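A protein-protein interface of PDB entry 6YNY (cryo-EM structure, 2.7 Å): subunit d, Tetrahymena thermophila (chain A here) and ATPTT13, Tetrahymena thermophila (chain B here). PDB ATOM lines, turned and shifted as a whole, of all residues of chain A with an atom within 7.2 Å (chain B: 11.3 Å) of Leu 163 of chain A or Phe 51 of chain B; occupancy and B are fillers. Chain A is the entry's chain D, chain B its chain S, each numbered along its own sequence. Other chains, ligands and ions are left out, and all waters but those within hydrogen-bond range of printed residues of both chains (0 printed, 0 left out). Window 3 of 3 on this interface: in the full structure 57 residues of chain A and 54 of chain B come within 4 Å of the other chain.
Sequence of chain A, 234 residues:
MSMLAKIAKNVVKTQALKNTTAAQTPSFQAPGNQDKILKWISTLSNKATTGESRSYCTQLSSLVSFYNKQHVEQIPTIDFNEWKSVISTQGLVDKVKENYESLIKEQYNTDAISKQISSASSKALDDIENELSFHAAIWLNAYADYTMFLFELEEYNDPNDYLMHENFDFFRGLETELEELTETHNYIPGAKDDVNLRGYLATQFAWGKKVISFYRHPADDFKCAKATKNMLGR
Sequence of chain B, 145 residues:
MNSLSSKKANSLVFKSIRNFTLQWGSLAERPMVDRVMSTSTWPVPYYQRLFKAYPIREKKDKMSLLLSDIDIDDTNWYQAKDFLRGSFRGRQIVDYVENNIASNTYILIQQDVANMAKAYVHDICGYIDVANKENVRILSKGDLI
The side-chain hydroxyl (OH) of Tyr 54 of chain B sits at hydrogen-bond distance from the side-chain carboxylate (OD2) of Asp 169 of chain A. The backbone carbonyl oxygen (O) of Asp 161 of chain A is in hydrogen-bond range of the backbone NH (N) of Lys 52 of chain B. NH2 of Arg 57 of chain B is in salt-bridge range of OD1 of Asp 169 of chain A (2.6 Å).
Asn 160 of chain A touches Phe 51 of chain B (O to CE1, 3.9 Å). Asp 161 of chain A touches Leu 50 of chain B (CA to O, 3.9 Å). O of Asp 161 of chain A touches CA of Phe 51 of chain B, 3.2 Å away. Tyr 162 of chain A touches Phe 51 of chain B (O to CD1, 3.5 Å). Tyr 162 of chain A touches Lys 52 of chain B. Lys 52 of chain B touches Leu 163 of chain A. His 165 of chain A touches Tyr 54 of chain B (CD2 to CD2, 3.6 Å). OE2 of Glu 166 of chain A touches CE of Lys 52 of chain B, at 3.4 Å. Glu 166 of chain A touches Tyr 54 of chain B. Phe 170 of chain A touches Lys 60 of chain B.
Printed residues of chain B within 4 Å of Leu 163 of chain A: Phe 51 and Lys 52. Phe 51 of chain B touches just these residues of chain A: Asn 160, Asp 161, Tyr 162 and Leu 163. Of chain B, only Leu 50 (3.9 Å), Phe 51 (3.2 Å) and Lys 52 (2.8 Å) come within 4 Å of Asp 161 of chain A. Of chain B, only Tyr 54 and Arg 57 come within 4 Å of His 165 of chain A. Glu 166 of chain A touches just these residues of chain B: Lys 52 (3.4 Å) and Tyr 54 (3.4 Å). Of the printed residues of chain A, Arg 57 of chain B touches His 165 and Asp 169. Printed residues of chain A within 4 Å of Tyr 54 of chain B: His 165, Glu 166 and Asp 169. Printed residues of chain A within 4 Å of Leu 50 of chain B: Asp 161 (3.9 Å). Of the printed residues of chain B, Phe 170 of chain A touches Lys 60 (3.8 Å). Printed residues of chain A within 4 Å of Lys 52 of chain B: Asp 161 (2.8 Å), Tyr 162 (3.6 Å), Leu 163 (3.8 Å) and Glu 166 (3.4 Å). Phe 168 of chain A touches none of the printed residues of chain B. Tyr 47 of chain B touches none of the printed residues of chain A. The nearest residue of chain B that does not touch Leu 163 of chain A is Tyr 54 of chain B (4.4 Å). The nearest residue of chain A that does not touch Phe 51 of chain B is Met 164 of chain A (6.0 Å). The nearest printed residue of chain A that does not touch Tyr 54 of chain B is Leu 163 of chain A (4.4 Å).
Of the 12 printed residues of chain B, 6 touch a printed residue of chain A. Printed residues of chain A that touch a printed residue of chain B: Asn 160, Asp 161, Tyr 162, Leu 163, His 165, Glu 166, Asp 169 and Phe 170. Hydrophobic or aromatic side chains of chain A within 4 Å of the printed part of chain B: Tyr 162, Leu 163, His 165 and Phe 170. Among the printed residues, Asp or Glu carboxylates within 4 Å of a Lys or Arg side-chain nitrogen of the other chain: Asp 169 of chain A with Arg 57 of chain B (2.6 Å).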
ATOM      1  N   PRO A 159     -26.674 -16.695   9.454  1.00  0.00           N
ATOM      2  CA  PRO A 159     -25.786 -17.546  10.260  1.00  0.00           C
ATOM      3  C   PRO A 159     -24.377 -17.004  10.378  1.00  0.00           C
ATOM      4  O   PRO A 159     -23.693 -17.272  11.374  1.00  0.00           O
ATOM      5  CB  PRO A 159     -25.815 -18.878   9.505  1.00  0.00           C
ATOM      6  CG  PRO A 159     -27.100 -18.877   8.791  1.00  0.00           C
ATOM      7  CD  PRO A 159     -27.389 -17.465   8.427  1.00  0.00           C
ATOM      8  N   ASN A 160     -23.915 -16.255   9.381  1.00  0.00           N
ATOM      9  CA  ASN A 160     -22.577 -15.688   9.391  1.00  0.00           C
ATOM     10  C   ASN A 160     -22.434 -14.526  10.359  1.00  0.00           C
ATOM     11  O   ASN A 160     -21.323 -14.013  10.521  1.00  0.00           O
ATOM     12  CB  ASN A 160     -22.207 -15.237   7.978  1.00  0.00           C
ATOM     13  CG  ASN A 160     -22.067 -16.393   7.017  1.00  0.00           C
ATOM     14  OD1 ASN A 160     -21.487 -17.426   7.349  1.00  0.00           O
ATOM     15  ND2 ASN A 160     -22.605 -16.232   5.821  1.00  0.00           N
ATOM     16  N   ASP A 161     -23.519 -14.107  11.006  1.00  0.00           N
ATOM     17  CA  ASP A 161     -23.491 -13.007  11.956  1.00  0.00           C
ATOM     18  C   ASP A 161     -23.577 -13.476  13.399  1.00  0.00           C
ATOM     19  O   ASP A 161     -23.572 -12.642  14.309  1.00  0.00           O
ATOM     20  CB  ASP A 161     -24.635 -12.034  11.660  1.00  0.00           C
ATOM     21  CG  ASP A 161     -24.599 -11.510  10.241  1.00  0.00           C
ATOM     22  OD1 ASP A 161     -23.654 -11.857   9.504  1.00  0.00           O
ATOM     23  OD2 ASP A 161     -25.515 -10.753   9.860  1.00  0.00           O
ATOM     24  N   TYR A 162     -23.660 -14.779  13.633  1.00  0.00           N
ATOM     25  CA  TYR A 162     -23.685 -15.340  14.974  1.00  0.00           C
ATOM     26  C   TYR A 162     -22.340 -15.963  15.311  1.00  0.00           C
ATOM     27  O   TYR A 162     -21.609 -16.426  14.433  1.00  0.00           O
ATOM     28  CB  TYR A 162     -24.770 -16.404  15.118  1.00  0.00           C
ATOM     29  CG  TYR A 162     -26.175 -15.898  14.977  1.00  0.00           C
ATOM     30  CD1 TYR A 162     -26.875 -16.065  13.798  1.00  0.00           C
ATOM     31  CD2 TYR A 162     -26.808 -15.263  16.028  1.00  0.00           C
ATOM     32  CE1 TYR A 162     -28.163 -15.610  13.670  1.00  0.00           C
ATOM     33  CE2 TYR A 162     -28.093 -14.803  15.908  1.00  0.00           C
ATOM     34  CZ  TYR A 162     -28.767 -14.980  14.727  1.00  0.00           C
ATOM     35  OH  TYR A 162     -30.054 -14.519  14.605  1.00  0.00           O
ATOM     36  N   LEU A 163     -22.023 -15.974  16.600  1.00  0.00           N
ATOM     37  CA  LEU A 163     -20.822 -16.648  17.051  1.00  0.00           C
ATOM     38  C   LEU A 163     -21.000 -18.160  16.941  1.00  0.00           C
ATOM     39  O   LEU A 163     -22.100 -18.677  16.738  1.00  0.00           O
ATOM     40  CB  LEU A 163     -20.487 -16.249  18.486  1.00  0.00           C
ATOM     41  CG  LEU A 163     -20.065 -14.794  18.694  1.00  0.00           C
ATOM     42  CD1 LEU A 163     -19.885 -14.487  20.163  1.00  0.00           C
ATOM     43  CD2 LEU A 163     -18.789 -14.504  17.941  1.00  0.00           C
ATOM     44  N   MET A 164     -19.886 -18.871  17.082  1.00  0.00           N
ATOM     45  CA  MET A 164     -19.894 -20.318  16.914  1.00  0.00           C
ATOM     46  C   MET A 164     -20.788 -20.989  17.949  1.00  0.00           C
ATOM     47  O   MET A 164     -21.714 -21.730  17.603  1.00  0.00           O
ATOM     48  CB  MET A 164     -18.462 -20.838  17.007  1.00  0.00           C
ATOM     49  CG  MET A 164     -18.317 -22.326  16.916  1.00  0.00           C
ATOM     50  SD  MET A 164     -18.455 -23.153  18.502  1.00  0.00           S
ATOM     51  CE  MET A 164     -17.635 -24.679  18.091  1.00  0.00           C
ATOM     52  N   HIS A 165     -20.524 -20.741  19.230  1.00  0.00           N
ATOM     53  CA  HIS A 165     -21.277 -21.409  20.283  1.00  0.00           C
ATOM     54  C   HIS A 165     -22.720 -20.936  20.374  1.00  0.00           C
ATOM     55  O   HIS A 165     -23.522 -21.595  21.041  1.00  0.00           O
ATOM     56  CB  HIS A 165     -20.576 -21.220  21.628  1.00  0.00           C
ATOM     57  CG  HIS A 165     -20.405 -19.792  22.033  1.00  0.00           C
ATOM     58  ND1 HIS A 165     -19.445 -18.972  21.483  1.00  0.00           N
ATOM     59  CD2 HIS A 165     -21.061 -19.042  22.947  1.00  0.00           C
ATOM     60  CE1 HIS A 165     -19.524 -17.776  22.034  1.00  0.00           C
ATOM     61  NE2 HIS A 165     -20.496 -17.792  22.926  1.00  0.00           N
ATOM     62  N   GLU A 166     -23.070 -19.824  19.730  1.00  0.00           N
ATOM     63  CA  GLU A 166     -24.460 -19.387  19.726  1.00  0.00           C
ATOM     64  C   GLU A 166     -25.261 -20.096  18.642  1.00  0.00           C
ATOM     65  O   GLU A 166     -26.432 -20.428  18.850  1.00  0.00           O
ATOM     66  CB  GLU A 166     -24.534 -17.874  19.535  1.00  0.00           C
ATOM     67  CG  GLU A 166     -25.927 -17.298  19.681  1.00  0.00           C
ATOM     68  CD  GLU A 166     -25.946 -15.787  19.690  1.00  0.00           C
ATOM     69  OE1 GLU A 166     -24.901 -15.173  19.388  1.00  0.00           O
ATOM     70  OE2 GLU A 166     -27.007 -15.213  20.004  1.00  0.00           O
ATOM     71  N   ASN A 167     -24.647 -20.338  17.484  1.00  0.00           N
ATOM     72  CA  ASN A 167     -25.327 -21.088  16.434  1.00  0.00           C
ATOM     73  C   ASN A 167     -25.651 -22.504  16.886  1.00  0.00           C
ATOM     74  O   ASN A 167     -26.732 -23.024  16.593  1.00  0.00           O
ATOM     75  CB  ASN A 167     -24.467 -21.118  15.175  1.00  0.00           C
ATOM     76  CG  ASN A 167     -24.889 -20.089  14.156  1.00  0.00           C
ATOM     77  OD1 ASN A 167     -26.058 -19.720  14.071  1.00  0.00           O
ATOM     78  ND2 ASN A 167     -23.938 -19.628  13.367  1.00  0.00           N
ATOM     79  N   PHE A 168     -24.720 -23.150  17.587  1.00  0.00           N
ATOM     80  CA  PHE A 168     -24.978 -24.490  18.099  1.00  0.00           C
ATOM     81  C   PHE A 168     -26.152 -24.509  19.066  1.00  0.00           C
ATOM     82  O   PHE A 168     -26.820 -25.539  19.207  1.00  0.00           O
ATOM     83  CB  PHE A 168     -23.727 -25.041  18.780  1.00  0.00           C
ATOM     84  CG  PHE A 168     -22.748 -25.669  17.838  1.00  0.00           C
ATOM     85  CD1 PHE A 168     -21.798 -24.907  17.196  1.00  0.00           C
ATOM     86  CD2 PHE A 168     -22.771 -27.027  17.601  1.00  0.00           C
ATOM     87  CE1 PHE A 168     -20.899 -25.485  16.335  1.00  0.00           C
ATOM     88  CE2 PHE A 168     -21.872 -27.606  16.742  1.00  0.00           C
ATOM     89  CZ  PHE A 168     -20.937 -26.833  16.109  1.00  0.00           C
ATOM     90  N   ASP A 169     -26.425 -23.390  19.735  1.00  0.00           N
ATOM     91  CA  ASP A 169     -27.549 -23.340  20.664  1.00  0.00           C
ATOM     92  C   ASP A 169     -28.881 -23.245  19.934  1.00  0.00           C
ATOM     93  O   ASP A 169     -29.881 -23.809  20.392  1.00  0.00           O
ATOM     94  CB  ASP A 169     -27.379 -22.170  21.625  1.00  0.00           C
ATOM     95  CG  ASP A 169     -26.220 -22.364  22.573  1.00  0.00           C
ATOM     96  OD1 ASP A 169     -25.506 -23.379  22.442  1.00  0.00           O
ATOM     97  OD2 ASP A 169     -26.020 -21.505  23.455  1.00  0.00           O
ATOM     98  N   PHE A 170     -28.923 -22.529  18.811  1.00  0.00           N
ATOM     99  CA  PHE A 170     -30.115 -22.563  17.973  1.00  0.00           C
ATOM    100  C   PHE A 170     -30.389 -23.978  17.485  1.00  0.00           C
ATOM    101  O   PHE A 170     -31.532 -24.446  17.513  1.00  0.00           O
ATOM    102  CB  PHE A 170     -29.960 -21.618  16.788  1.00  0.00           C
ATOM    103  CG  PHE A 170     -30.129 -20.173  17.133  1.00  0.00           C
ATOM    104  CD1 PHE A 170     -31.383 -19.644  17.356  1.00  0.00           C
ATOM    105  CD2 PHE A 170     -29.036 -19.337  17.210  1.00  0.00           C
ATOM    106  CE1 PHE A 170     -31.540 -18.317  17.663  1.00  0.00           C
ATOM    107  CE2 PHE A 170     -29.189 -18.009  17.517  1.00  0.00           C
ATOM    108  CZ  PHE A 170     -30.443 -17.497  17.741  1.00  0.00           C
ATOM    109  N   TYR B  47     -18.206   1.924  12.853  1.00  0.00           N
ATOM    110  CA  TYR B  47     -17.989   0.517  13.148  1.00  0.00           C
ATOM    111  C   TYR B  47     -19.084  -0.342  12.536  1.00  0.00           C
ATOM    112  O   TYR B  47     -20.275  -0.085  12.727  1.00  0.00           O
ATOM    113  CB  TYR B  47     -17.926   0.297  14.653  1.00  0.00           C
ATOM    114  CG  TYR B  47     -17.322  -1.028  15.029  1.00  0.00           C
ATOM    115  CD1 TYR B  47     -15.952  -1.189  15.091  1.00  0.00           C
ATOM    116  CD2 TYR B  47     -18.120  -2.121  15.311  1.00  0.00           C
ATOM    117  CE1 TYR B  47     -15.395  -2.395  15.426  1.00  0.00           C
ATOM    118  CE2 TYR B  47     -17.571  -3.331  15.647  1.00  0.00           C
ATOM    119  CZ  TYR B  47     -16.206  -3.463  15.702  1.00  0.00           C
ATOM    120  OH  TYR B  47     -15.650  -4.670  16.037  1.00  0.00           O
ATOM    121  N   GLN B  48     -18.671  -1.366  11.801  1.00  0.00           N
ATOM    122  CA  GLN B  48     -19.582  -2.351  11.240  1.00  0.00           C
ATOM    123  C   GLN B  48     -19.528  -3.603  12.101  1.00  0.00           C
ATOM    124  O   GLN B  48     -18.464  -4.208  12.262  1.00  0.00           O
ATOM    125  CB  GLN B  48     -19.220  -2.666   9.790  1.00  0.00           C
ATOM    126  CG  GLN B  48     -20.056  -3.764   9.156  1.00  0.00           C
ATOM    127  CD  GLN B  48     -21.540  -3.500   9.238  1.00  0.00           C
ATOM    128  OE1 GLN B  48     -21.987  -2.362   9.103  1.00  0.00           O
ATOM    129  NE2 GLN B  48     -22.318  -4.553   9.475  1.00  0.00           N
ATOM    130  N   ARG B  49     -20.674  -3.979  12.654  1.00  0.00           N
ATOM    131  CA  ARG B  49     -20.739  -5.101  13.576  1.00  0.00           C
ATOM    132  C   ARG B  49     -20.429  -6.400  12.849  1.00  0.00           C
ATOM    133  O   ARG B  49     -20.946  -6.656  11.758  1.00  0.00           O
ATOM    134  CB  ARG B  49     -22.118  -5.159  14.225  1.00  0.00           C
ATOM    135  CG  ARG B  49     -22.320  -4.111  15.292  1.00  0.00           C
ATOM    136  CD  ARG B  49     -21.668  -4.525  16.584  1.00  0.00           C
ATOM    137  NE  ARG B  49     -22.585  -5.266  17.439  1.00  0.00           N
ATOM    138  CZ  ARG B  49     -22.209  -6.167  18.336  1.00  0.00           C
ATOM    139  NH1 ARG B  49     -20.930  -6.459  18.507  1.00  0.00           N
ATOM    140  NH2 ARG B  49     -23.122  -6.786  19.063  1.00  0.00           N
ATOM    141  N   LEU B  50     -19.568  -7.215  13.453  1.00  0.00           N
ATOM    142  CA  LEU B  50     -19.191  -8.500  12.884  1.00  0.00           C
ATOM    143  C   LEU B  50     -20.131  -9.609  13.334  1.00  0.00           C
ATOM    144  O   LEU B  50     -20.659 -10.356  12.505  1.00  0.00           O
ATOM    145  CB  LEU B  50     -17.759  -8.844  13.289  1.00  0.00           C
ATOM    146  CG  LEU B  50     -16.709  -7.806  12.920  1.00  0.00           C
ATOM    147  CD1 LEU B  50     -15.498  -7.967  13.797  1.00  0.00           C
ATOM    148  CD2 LEU B  50     -16.339  -7.938  11.465  1.00  0.00           C
ATOM    149  N   PHE B  51     -20.343  -9.727  14.640  1.00  0.00           N
ATOM    150  CA  PHE B  51     -21.134 -10.799  15.210  1.00  0.00           C
ATOM    151  C   PHE B  51     -22.182 -10.222  16.143  1.00  0.00           C
ATOM    152  O   PHE B  51     -22.196  -9.027  16.449  1.00  0.00           O
ATOM    153  CB  PHE B  51     -20.266 -11.797  15.986  1.00  0.00           C
ATOM    154  CG  PHE B  51     -19.277 -12.525  15.145  1.00  0.00           C
ATOM    155  CD1 PHE B  51     -19.686 -13.512  14.276  1.00  0.00           C
ATOM    156  CD2 PHE B  51     -17.930 -12.243  15.247  1.00  0.00           C
ATOM    157  CE1 PHE B  51     -18.774 -14.191  13.509  1.00  0.00           C
ATOM    158  CE2 PHE B  51     -17.014 -12.918  14.484  1.00  0.00           C
ATOM    159  CZ  PHE B  51     -17.435 -13.895  13.612  1.00  0.00           C
ATOM    160  N   LYS B  52     -23.066 -11.100  16.596  1.00  0.00           N
ATOM    161  CA  LYS B  52     -24.017 -10.778  17.643  1.00  0.00           C
ATOM    162  C   LYS B  52     -23.392 -11.097  18.991  1.00  0.00           C
ATOM    163  O   LYS B  52     -22.798 -12.163  19.172  1.00  0.00           O
ATOM    164  CB  LYS B  52     -25.312 -11.565  17.459  1.00  0.00           C
ATOM    165  CG  LYS B  52     -26.348 -11.306  18.521  1.00  0.00           C
ATOM    166  CD  LYS B  52     -27.498 -12.266  18.401  1.00  0.00           C
ATOM    167  CE  LYS B  52     -28.401 -12.166  19.597  1.00  0.00           C
ATOM    168  NZ  LYS B  52     -28.993 -10.811  19.686  1.00  0.00           N
ATOM    169  N   ALA B  53     -23.518 -10.169  19.930  1.00  0.00           N
ATOM    170  CA  ALA B  53     -23.007 -10.395  21.270  1.00  0.00           C
ATOM    171  C   ALA B  53     -23.809 -11.494  21.954  1.00  0.00           C
ATOM    172  O   ALA B  53     -25.041 -11.505  21.898  1.00  0.00           O
ATOM    173  CB  ALA B  53     -23.069  -9.108  22.080  1.00  0.00           C
ATOM    174  N   TYR B  54     -23.104 -12.419  22.597  1.00  0.00           N
ATOM    175  CA  TYR B  54     -23.717 -13.545  23.300  1.00  0.00           C
ATOM    176  C   TYR B  54     -23.037 -13.683  24.653  1.00  0.00           C
ATOM    177  O   TYR B  54     -22.211 -14.577  24.870  1.00  0.00           O
ATOM    178  CB  TYR B  54     -23.608 -14.828  22.476  1.00  0.00           C
ATOM    179  CG  TYR B  54     -24.561 -15.925  22.889  1.00  0.00           C
ATOM    180  CD1 TYR B  54     -25.895 -15.655  23.138  1.00  0.00           C
ATOM    181  CD2 TYR B  54     -24.133 -17.235  22.997  1.00  0.00           C
ATOM    182  CE1 TYR B  54     -26.766 -16.651  23.505  1.00  0.00           C
ATOM    183  CE2 TYR B  54     -24.998 -18.238  23.361  1.00  0.00           C
ATOM    184  CZ  TYR B  54     -26.314 -17.942  23.613  1.00  0.00           C
ATOM    185  OH  TYR B  54     -27.181 -18.942  23.977  1.00  0.00           O
ATOM    186  N   PRO B  55     -23.355 -12.789  25.591  1.00  0.00           N
ATOM    187  CA  PRO B  55     -22.635 -12.794  26.871  1.00  0.00           C
ATOM    188  C   PRO B  55     -23.033 -13.935  27.782  1.00  0.00           C
ATOM    189  O   PRO B  55     -22.167 -14.537  28.428  1.00  0.00           O
ATOM    190  CB  PRO B  55     -23.006 -11.432  27.465  1.00  0.00           C
ATOM    191  CG  PRO B  55     -24.354 -11.156  26.914  1.00  0.00           C
ATOM    192  CD  PRO B  55     -24.382 -11.737  25.540  1.00  0.00           C
ATOM    193  N   ILE B  56     -24.322 -14.248  27.858  1.00  0.00           N
ATOM    194  CA  ILE B  56     -24.841 -15.276  28.749  1.00  0.00           C
ATOM    195  C   ILE B  56     -25.295 -16.454  27.903  1.00  0.00           C
ATOM    196  O   ILE B  56     -26.128 -16.301  27.003  1.00  0.00           O
ATOM    197  CB  ILE B  56     -25.990 -14.745  29.618  1.00  0.00           C
ATOM    198  CG1 ILE B  56     -25.538 -13.500  30.377  1.00  0.00           C
ATOM    199  CG2 ILE B  56     -26.439 -15.800  30.600  1.00  0.00           C
ATOM    200  CD1 ILE B  56     -26.608 -12.879  31.222  1.00  0.00           C
ATOM    201  N   ARG B  57     -24.749 -17.630  28.203  1.00  0.00           N
ATOM    202  CA  ARG B  57     -25.119 -18.873  27.530  1.00  0.00           C
ATOM    203  C   ARG B  57     -26.446 -19.351  28.108  1.00  0.00           C
ATOM    204  O   ARG B  57     -26.515 -20.234  28.965  1.00  0.00           O
ATOM    205  CB  ARG B  57     -24.027 -19.917  27.697  1.00  0.00           C
ATOM    206  CG  ARG B  57     -24.196 -21.121  26.806  1.00  0.00           C
ATOM    207  CD  ARG B  57     -23.494 -20.934  25.487  1.00  0.00           C
ATOM    208  NE  ARG B  57     -23.759 -22.053  24.591  1.00  0.00           N
ATOM    209  CZ  ARG B  57     -23.089 -23.199  24.603  1.00  0.00           C
ATOM    210  NH1 ARG B  57     -22.100 -23.393  25.460  1.00  0.00           N
ATOM    211  NH2 ARG B  57     -23.416 -24.157  23.749  1.00  0.00           N
ATOM    212  N   LYS B  60     -32.320 -21.574  25.437  1.00  0.00           N
ATOM    213  CA  LYS B  60     -33.359 -20.909  24.668  1.00  0.00           C
ATOM    214  C   LYS B  60     -34.666 -21.686  24.761  1.00  0.00           C
ATOM    215  O   LYS B  60     -34.708 -22.882  24.458  1.00  0.00           O
ATOM    216  CB  LYS B  60     -32.931 -20.772  23.209  1.00  0.00           C
ATOM    217  CG  LYS B  60     -31.615 -20.047  22.997  1.00  0.00           C
ATOM    218  CD  LYS B  60     -31.251 -20.016  21.527  1.00  0.00           C
ATOM    219  CE  LYS B  60     -29.920 -19.346  21.272  1.00  0.00           C
ATOM    220  NZ  LYS B  60     -29.962 -17.882  21.503  1.00  0.00           N
